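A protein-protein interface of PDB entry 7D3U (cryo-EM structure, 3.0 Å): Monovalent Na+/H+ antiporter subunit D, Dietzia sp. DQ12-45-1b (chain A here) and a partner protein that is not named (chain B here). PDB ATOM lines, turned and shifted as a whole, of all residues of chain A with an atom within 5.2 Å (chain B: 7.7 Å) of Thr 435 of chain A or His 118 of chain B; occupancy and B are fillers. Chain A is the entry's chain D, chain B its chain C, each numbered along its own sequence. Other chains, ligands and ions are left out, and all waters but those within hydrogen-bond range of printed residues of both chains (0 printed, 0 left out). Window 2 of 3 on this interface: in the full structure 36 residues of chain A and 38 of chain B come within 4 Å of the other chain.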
ATOM      1  N   GLY A 357     -26.148   6.922 -23.202  1.00  0.00           N
ATOM      2  CA  GLY A 357     -25.295   7.932 -22.619  1.00  0.00           C
ATOM      3  C   GLY A 357     -25.954   8.745 -21.529  1.00  0.00           C
ATOM      4  O   GLY A 357     -25.248   9.366 -20.725  1.00  0.00           O
ATOM      5  N   SER A 360     -25.375   5.775 -16.781  1.00  0.00           N
ATOM      6  CA  SER A 360     -23.994   5.335 -16.674  1.00  0.00           C
ATOM      7  C   SER A 360     -23.811   4.575 -15.372  1.00  0.00           C
ATOM      8  O   SER A 360     -24.489   4.845 -14.379  1.00  0.00           O
ATOM      9  CB  SER A 360     -23.023   6.519 -16.736  1.00  0.00           C
ATOM     10  OG  SER A 360     -23.075   7.153 -18.001  1.00  0.00           O
ATOM     11  N   GLY A 432     -19.125   2.979 -16.805  1.00  0.00           N
ATOM     12  CA  GLY A 432     -18.952   4.374 -16.457  1.00  0.00           C
ATOM     13  C   GLY A 432     -19.109   4.625 -14.974  1.00  0.00           C
ATOM     14  O   GLY A 432     -19.379   3.696 -14.207  1.00  0.00           O
ATOM     15  N   GLU A 433     -18.938   5.874 -14.553  1.00  0.00           N
ATOM     16  CA  GLU A 433     -19.161   6.094 -13.130  1.00  0.00           C
ATOM     17  C   GLU A 433     -20.634   6.383 -12.867  1.00  0.00           C
ATOM     18  O   GLU A 433     -21.267   7.121 -13.628  1.00  0.00           O
ATOM     19  CB  GLU A 433     -18.319   7.259 -12.624  1.00  0.00           C
ATOM     20  CG  GLU A 433     -16.843   6.946 -12.492  1.00  0.00           C
ATOM     21  CD  GLU A 433     -16.555   5.963 -11.380  1.00  0.00           C
ATOM     22  OE1 GLU A 433     -17.355   5.892 -10.423  1.00  0.00           O
ATOM     23  OE2 GLU A 433     -15.527   5.259 -11.460  1.00  0.00           O
ATOM     24  N   PRO A 434     -21.201   5.817 -11.805  1.00  0.00           N
ATOM     25  CA  PRO A 434     -22.615   6.073 -11.503  1.00  0.00           C
ATOM     26  C   PRO A 434     -22.873   7.530 -11.161  1.00  0.00           C
ATOM     27  O   PRO A 434     -22.429   8.022 -10.119  1.00  0.00           O
ATOM     28  CB  PRO A 434     -22.891   5.153 -10.307  1.00  0.00           C
ATOM     29  CG  PRO A 434     -21.798   4.140 -10.329  1.00  0.00           C
ATOM     30  CD  PRO A 434     -20.603   4.850 -10.873  1.00  0.00           C
ATOM     31  N   THR A 435     -23.580   8.223 -12.033  1.00  0.00           N
ATOM     32  CA  THR A 435     -23.935   9.619 -11.853  1.00  0.00           C
ATOM     33  C   THR A 435     -25.370   9.747 -11.361  1.00  0.00           C
ATOM     34  O   THR A 435     -26.234   8.944 -11.728  1.00  0.00           O
ATOM     35  CB  THR A 435     -23.787  10.396 -13.164  1.00  0.00           C
ATOM     36  OG1 THR A 435     -24.441   9.681 -14.218  1.00  0.00           O
ATOM     37  CG2 THR A 435     -22.321  10.582 -13.516  1.00  0.00           C
ATOM     38  N   PRO A 436     -25.655  10.750 -10.531  1.00  0.00           N
ATOM     39  CA  PRO A 436     -27.029  10.945 -10.043  1.00  0.00           C
ATOM     40  C   PRO A 436     -27.946  11.383 -11.176  1.00  0.00           C
ATOM     41  O   PRO A 436     -27.646  12.332 -11.903  1.00  0.00           O
ATOM     42  CB  PRO A 436     -26.876  12.041  -8.981  1.00  0.00           C
ATOM     43  CG  PRO A 436     -25.412  12.079  -8.660  1.00  0.00           C
ATOM     44  CD  PRO A 436     -24.719  11.708  -9.926  1.00  0.00           C
ATOM     45  N   THR A 437     -29.069  10.684 -11.321  1.00  0.00           N
ATOM     46  CA  THR A 437     -30.050  10.973 -12.354  1.00  0.00           C
ATOM     47  C   THR A 437     -31.403  11.274 -11.724  1.00  0.00           C
ATOM     48  O   THR A 437     -31.680  10.905 -10.580  1.00  0.00           O
ATOM     49  CB  THR A 437     -30.188   9.809 -13.343  1.00  0.00           C
ATOM     50  OG1 THR A 437     -31.000  10.214 -14.452  1.00  0.00           O
ATOM     51  CG2 THR A 437     -30.821   8.606 -12.667  1.00  0.00           C
ATOM     52  N   VAL A 520     -31.584  11.824  -7.874  1.00  0.00           N
ATOM     53  CA  VAL A 520     -31.449  10.710  -6.933  1.00  0.00           C
ATOM     54  C   VAL A 520     -30.001  10.235  -6.937  1.00  0.00           C
ATOM     55  O   VAL A 520     -29.431  10.029  -8.020  1.00  0.00           O
ATOM     56  CB  VAL A 520     -32.397   9.578  -7.307  1.00  0.00           C
ATOM     57  CG1 VAL A 520     -32.565   8.616  -6.143  1.00  0.00           C
ATOM     58  CG2 VAL A 520     -33.735  10.138  -7.735  1.00  0.00           C
ATOM     59  N   PRO A 522     -26.897   7.634  -6.837  1.00  0.00           N
ATOM     60  CA  PRO A 522     -26.856   6.296  -7.437  1.00  0.00           C
ATOM     61  C   PRO A 522     -27.169   5.214  -6.415  1.00  0.00           C
ATOM     62  O   PRO A 522     -26.648   5.215  -5.299  1.00  0.00           O
ATOM     63  CB  PRO A 522     -25.419   6.183  -7.954  1.00  0.00           C
ATOM     64  CG  PRO A 522     -24.954   7.594  -8.097  1.00  0.00           C
ATOM     65  CD  PRO A 522     -25.616   8.343  -6.989  1.00  0.00           C
ATOM     66  N   PRO B 114     -28.496  17.452 -22.008  1.00  0.00           N
ATOM     67  CA  PRO B 114     -27.494  17.503 -23.076  1.00  0.00           C
ATOM     68  C   PRO B 114     -26.129  17.008 -22.620  1.00  0.00           C
ATOM     69  O   PRO B 114     -25.771  17.061 -21.443  1.00  0.00           O
ATOM     70  CB  PRO B 114     -27.445  18.990 -23.433  1.00  0.00           C
ATOM     71  CG  PRO B 114     -27.777  19.676 -22.154  1.00  0.00           C
ATOM     72  CD  PRO B 114     -28.764  18.784 -21.439  1.00  0.00           C
ATOM     73  N   GLY B 115     -25.367  16.519 -23.595  1.00  0.00           N
ATOM     74  CA  GLY B 115     -24.036  16.007 -23.344  1.00  0.00           C
ATOM     75  C   GLY B 115     -24.024  14.569 -22.869  1.00  0.00           C
ATOM     76  O   GLY B 115     -23.120  13.802 -23.213  1.00  0.00           O
ATOM     77  N   GLY B 116     -25.023  14.193 -22.079  1.00  0.00           N
ATOM     78  CA  GLY B 116     -25.093  12.864 -21.506  1.00  0.00           C
ATOM     79  C   GLY B 116     -24.733  12.870 -20.035  1.00  0.00           C
ATOM     80  O   GLY B 116     -24.415  13.901 -19.435  1.00  0.00           O
ATOM     81  N   ALA B 117     -24.791  11.677 -19.444  1.00  0.00           N
ATOM     82  CA  ALA B 117     -24.412  11.524 -18.045  1.00  0.00           C
ATOM     83  C   ALA B 117     -22.926  11.754 -17.812  1.00  0.00           C
ATOM     84  O   ALA B 117     -22.507  11.857 -16.654  1.00  0.00           O
ATOM     85  CB  ALA B 117     -24.803  10.137 -17.541  1.00  0.00           C
ATOM     86  N   HIS B 118     -22.127  11.836 -18.873  1.00  0.00           N
ATOM     87  CA  HIS B 118     -20.695  12.114 -18.768  1.00  0.00           C
ATOM     88  C   HIS B 118     -20.305  13.062 -19.890  1.00  0.00           C
ATOM     89  O   HIS B 118     -19.808  12.640 -20.941  1.00  0.00           O
ATOM     90  CB  HIS B 118     -19.874  10.824 -18.827  1.00  0.00           C
ATOM     91  CG  HIS B 118     -19.860  10.058 -17.542  1.00  0.00           C
ATOM     92  ND1 HIS B 118     -19.334  10.571 -16.376  1.00  0.00           N
ATOM     93  CD2 HIS B 118     -20.304   8.816 -17.240  1.00  0.00           C
ATOM     94  CE1 HIS B 118     -19.456   9.678 -15.411  1.00  0.00           C
ATOM     95  NE2 HIS B 118     -20.042   8.604 -15.908  1.00  0.00           N
ATOM     96  N   PRO B 119     -20.522  14.366 -19.701  1.00  0.00           N
ATOM     97  CA  PRO B 119     -20.154  15.332 -20.747  1.00  0.00           C
ATOM     98  C   PRO B 119     -18.657  15.521 -20.900  1.00  0.00           C
ATOM     99  O   PRO B 119     -18.234  16.213 -21.834  1.00  0.00           O
ATOM    100  CB  PRO B 119     -20.831  16.624 -20.279  1.00  0.00           C
ATOM    101  CG  PRO B 119     -20.883  16.488 -18.798  1.00  0.00           C
ATOM    102  CD  PRO B 119     -21.094  15.025 -18.514  1.00  0.00           C
ATOM    103  N   GLU B 120     -17.847  14.936 -20.020  1.00  0.00           N
ATOM    104  CA  GLU B 120     -16.399  15.076 -20.093  1.00  0.00           C
ATOM    105  C   GLU B 120     -15.746  14.012 -20.962  1.00  0.00           C
ATOM    106  O   GLU B 120     -14.645  14.235 -21.476  1.00  0.00           O
ATOM    107  CB  GLU B 120     -15.795  15.025 -18.689  1.00  0.00           C
ATOM    108  CG  GLU B 120     -16.179  13.787 -17.898  1.00  0.00           C
ATOM    109  CD  GLU B 120     -17.261  14.064 -16.872  1.00  0.00           C
ATOM    110  OE1 GLU B 120     -17.802  15.189 -16.868  1.00  0.00           O
ATOM    111  OE2 GLU B 120     -17.569  13.157 -16.071  1.00  0.00           O
ATOM    112  N   ASP B 121     -16.397  12.859 -21.135  1.00  0.00           N
ATOM    113  CA  ASP B 121     -15.856  11.739 -21.902  1.00  0.00           C
ATOM    114  C   ASP B 121     -16.799  11.433 -23.060  1.00  0.00           C
ATOM    115  O   ASP B 121     -17.620  10.506 -22.977  1.00  0.00           O
ATOM    116  CB  ASP B 121     -15.658  10.510 -21.017  1.00  0.00           C
ATOM    117  CG  ASP B 121     -15.055   9.339 -21.770  1.00  0.00           C
ATOM    118  OD1 ASP B 121     -14.316   9.576 -22.749  1.00  0.00           O
ATOM    119  OD2 ASP B 121     -15.319   8.182 -21.381  1.00  0.00           O
ATOM    120  N   PRO B 122     -16.716  12.189 -24.153  1.00  0.00           N
ATOM    121  CA  PRO B 122     -17.530  11.864 -25.329  1.00  0.00           C
ATOM    122  C   PRO B 122     -17.018  10.605 -26.009  1.00  0.00           C
ATOM    123  O   PRO B 122     -15.811  10.402 -26.154  1.00  0.00           O
ATOM    124  CB  PRO B 122     -17.366  13.094 -26.226  1.00  0.00           C
ATOM    125  CG  PRO B 122     -16.044  13.654 -25.840  1.00  0.00           C
ATOM    126  CD  PRO B 122     -15.894  13.392 -24.366  1.00  0.00           C
ATOM    127  N   GLU B 123     -17.952   9.755 -26.419  1.00  0.00           N
ATOM    128  CA  GLU B 123     -17.584   8.503 -27.062  1.00  0.00           C
ATOM    129  C   GLU B 123     -16.883   8.784 -28.387  1.00  0.00           C
ATOM    130  O   GLU B 123     -17.422   9.524 -29.222  1.00  0.00           O
ATOM    131  CB  GLU B 123     -18.821   7.636 -27.291  1.00  0.00           C
ATOM    132  CG  GLU B 123     -19.586   7.304 -26.021  1.00  0.00           C
ATOM    133  CD  GLU B 123     -19.167   5.980 -25.417  1.00  0.00           C
ATOM    134  OE1 GLU B 123     -18.530   5.989 -24.342  1.00  0.00           O
ATOM    135  OE2 GLU B 123     -19.473   4.928 -26.019  1.00  0.00           O
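Gly 116 of chain B touches Gly 357 of chain A (CA to O, 3.6 Å).
Ser 360 of chain A touches Ala 117 of chain B (OG to CB, 3.5 Å).
CD2 of His 118 of chain B touches OG of Ser 360 of chain A, 3.3 Å away.
Thr 435 of chain A touches Ala 117 of chain B.
His 118 of chain B touches Thr 435 of chain A (CE1 to CG2, 3.6 Å).
Thr 435 of chain A touches just these residues of chain B: Ala 117 (3.4 Å) and His 118 (3.6 Å).
His 118 of chain B touches just these residues of chain A: Ser 360 (3.3 Å), Glu 433 (3.0 Å) and Thr 435 (3.6 Å).
No residue of chain B comes within 4 Å of Pro 436 of chain A.
Of the printed residues of chain B, Gly 357 of chain A touches Gly 116 (3.6 Å) and Ala 117 (2.7 Å).
Of the printed residues of chain A, Gly 116 of chain B touches Gly 357.
Of the printed residues of chain B, Glu 433 of chain A touches His 118 (3.0 Å).
Pro 522 of chain A touches none of the printed residues of chain B.
The nearest residue of chain B that does not touch Thr 435 of chain A is Glu 120 of chain B (6.0 Å).
The nearest residue of chain A that does not touch His 118 of chain B is Gly 432 of chain A (4.2 Å).
The nearest printed residue of chain A that does not touch Gly 116 of chain B is Ser 360 of chain A (6.3 Å).
NE2 of His 118 of chain B is in hydrogen-bond range of O of Glu 433 of chain A, at 3.0 Å.
N of Ala 117 of chain B sits at hydrogen-bond distance from O of Gly 357 of chain A (2.7 Å).
OE2 of Glu 120 of chain B is in hydrogen-bond range of ND1 of His 118 of chain B (3.1 Å).
Printed residues of chain A that touch a printed residue of chain B: Gly 357, Ser 360, Glu 433 and Thr 435.
Of the 10 printed residues of chain B, 3 touch a printed residue of chain A.
Printed residues of chain B that touch a printed residue of chain A: Gly 116, Ala 117 and His 118.
Among the printed residues, no Asp or Glu carboxylate lies within 4 Å of a Lys or Arg side-chain nitrogen of the other chain.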
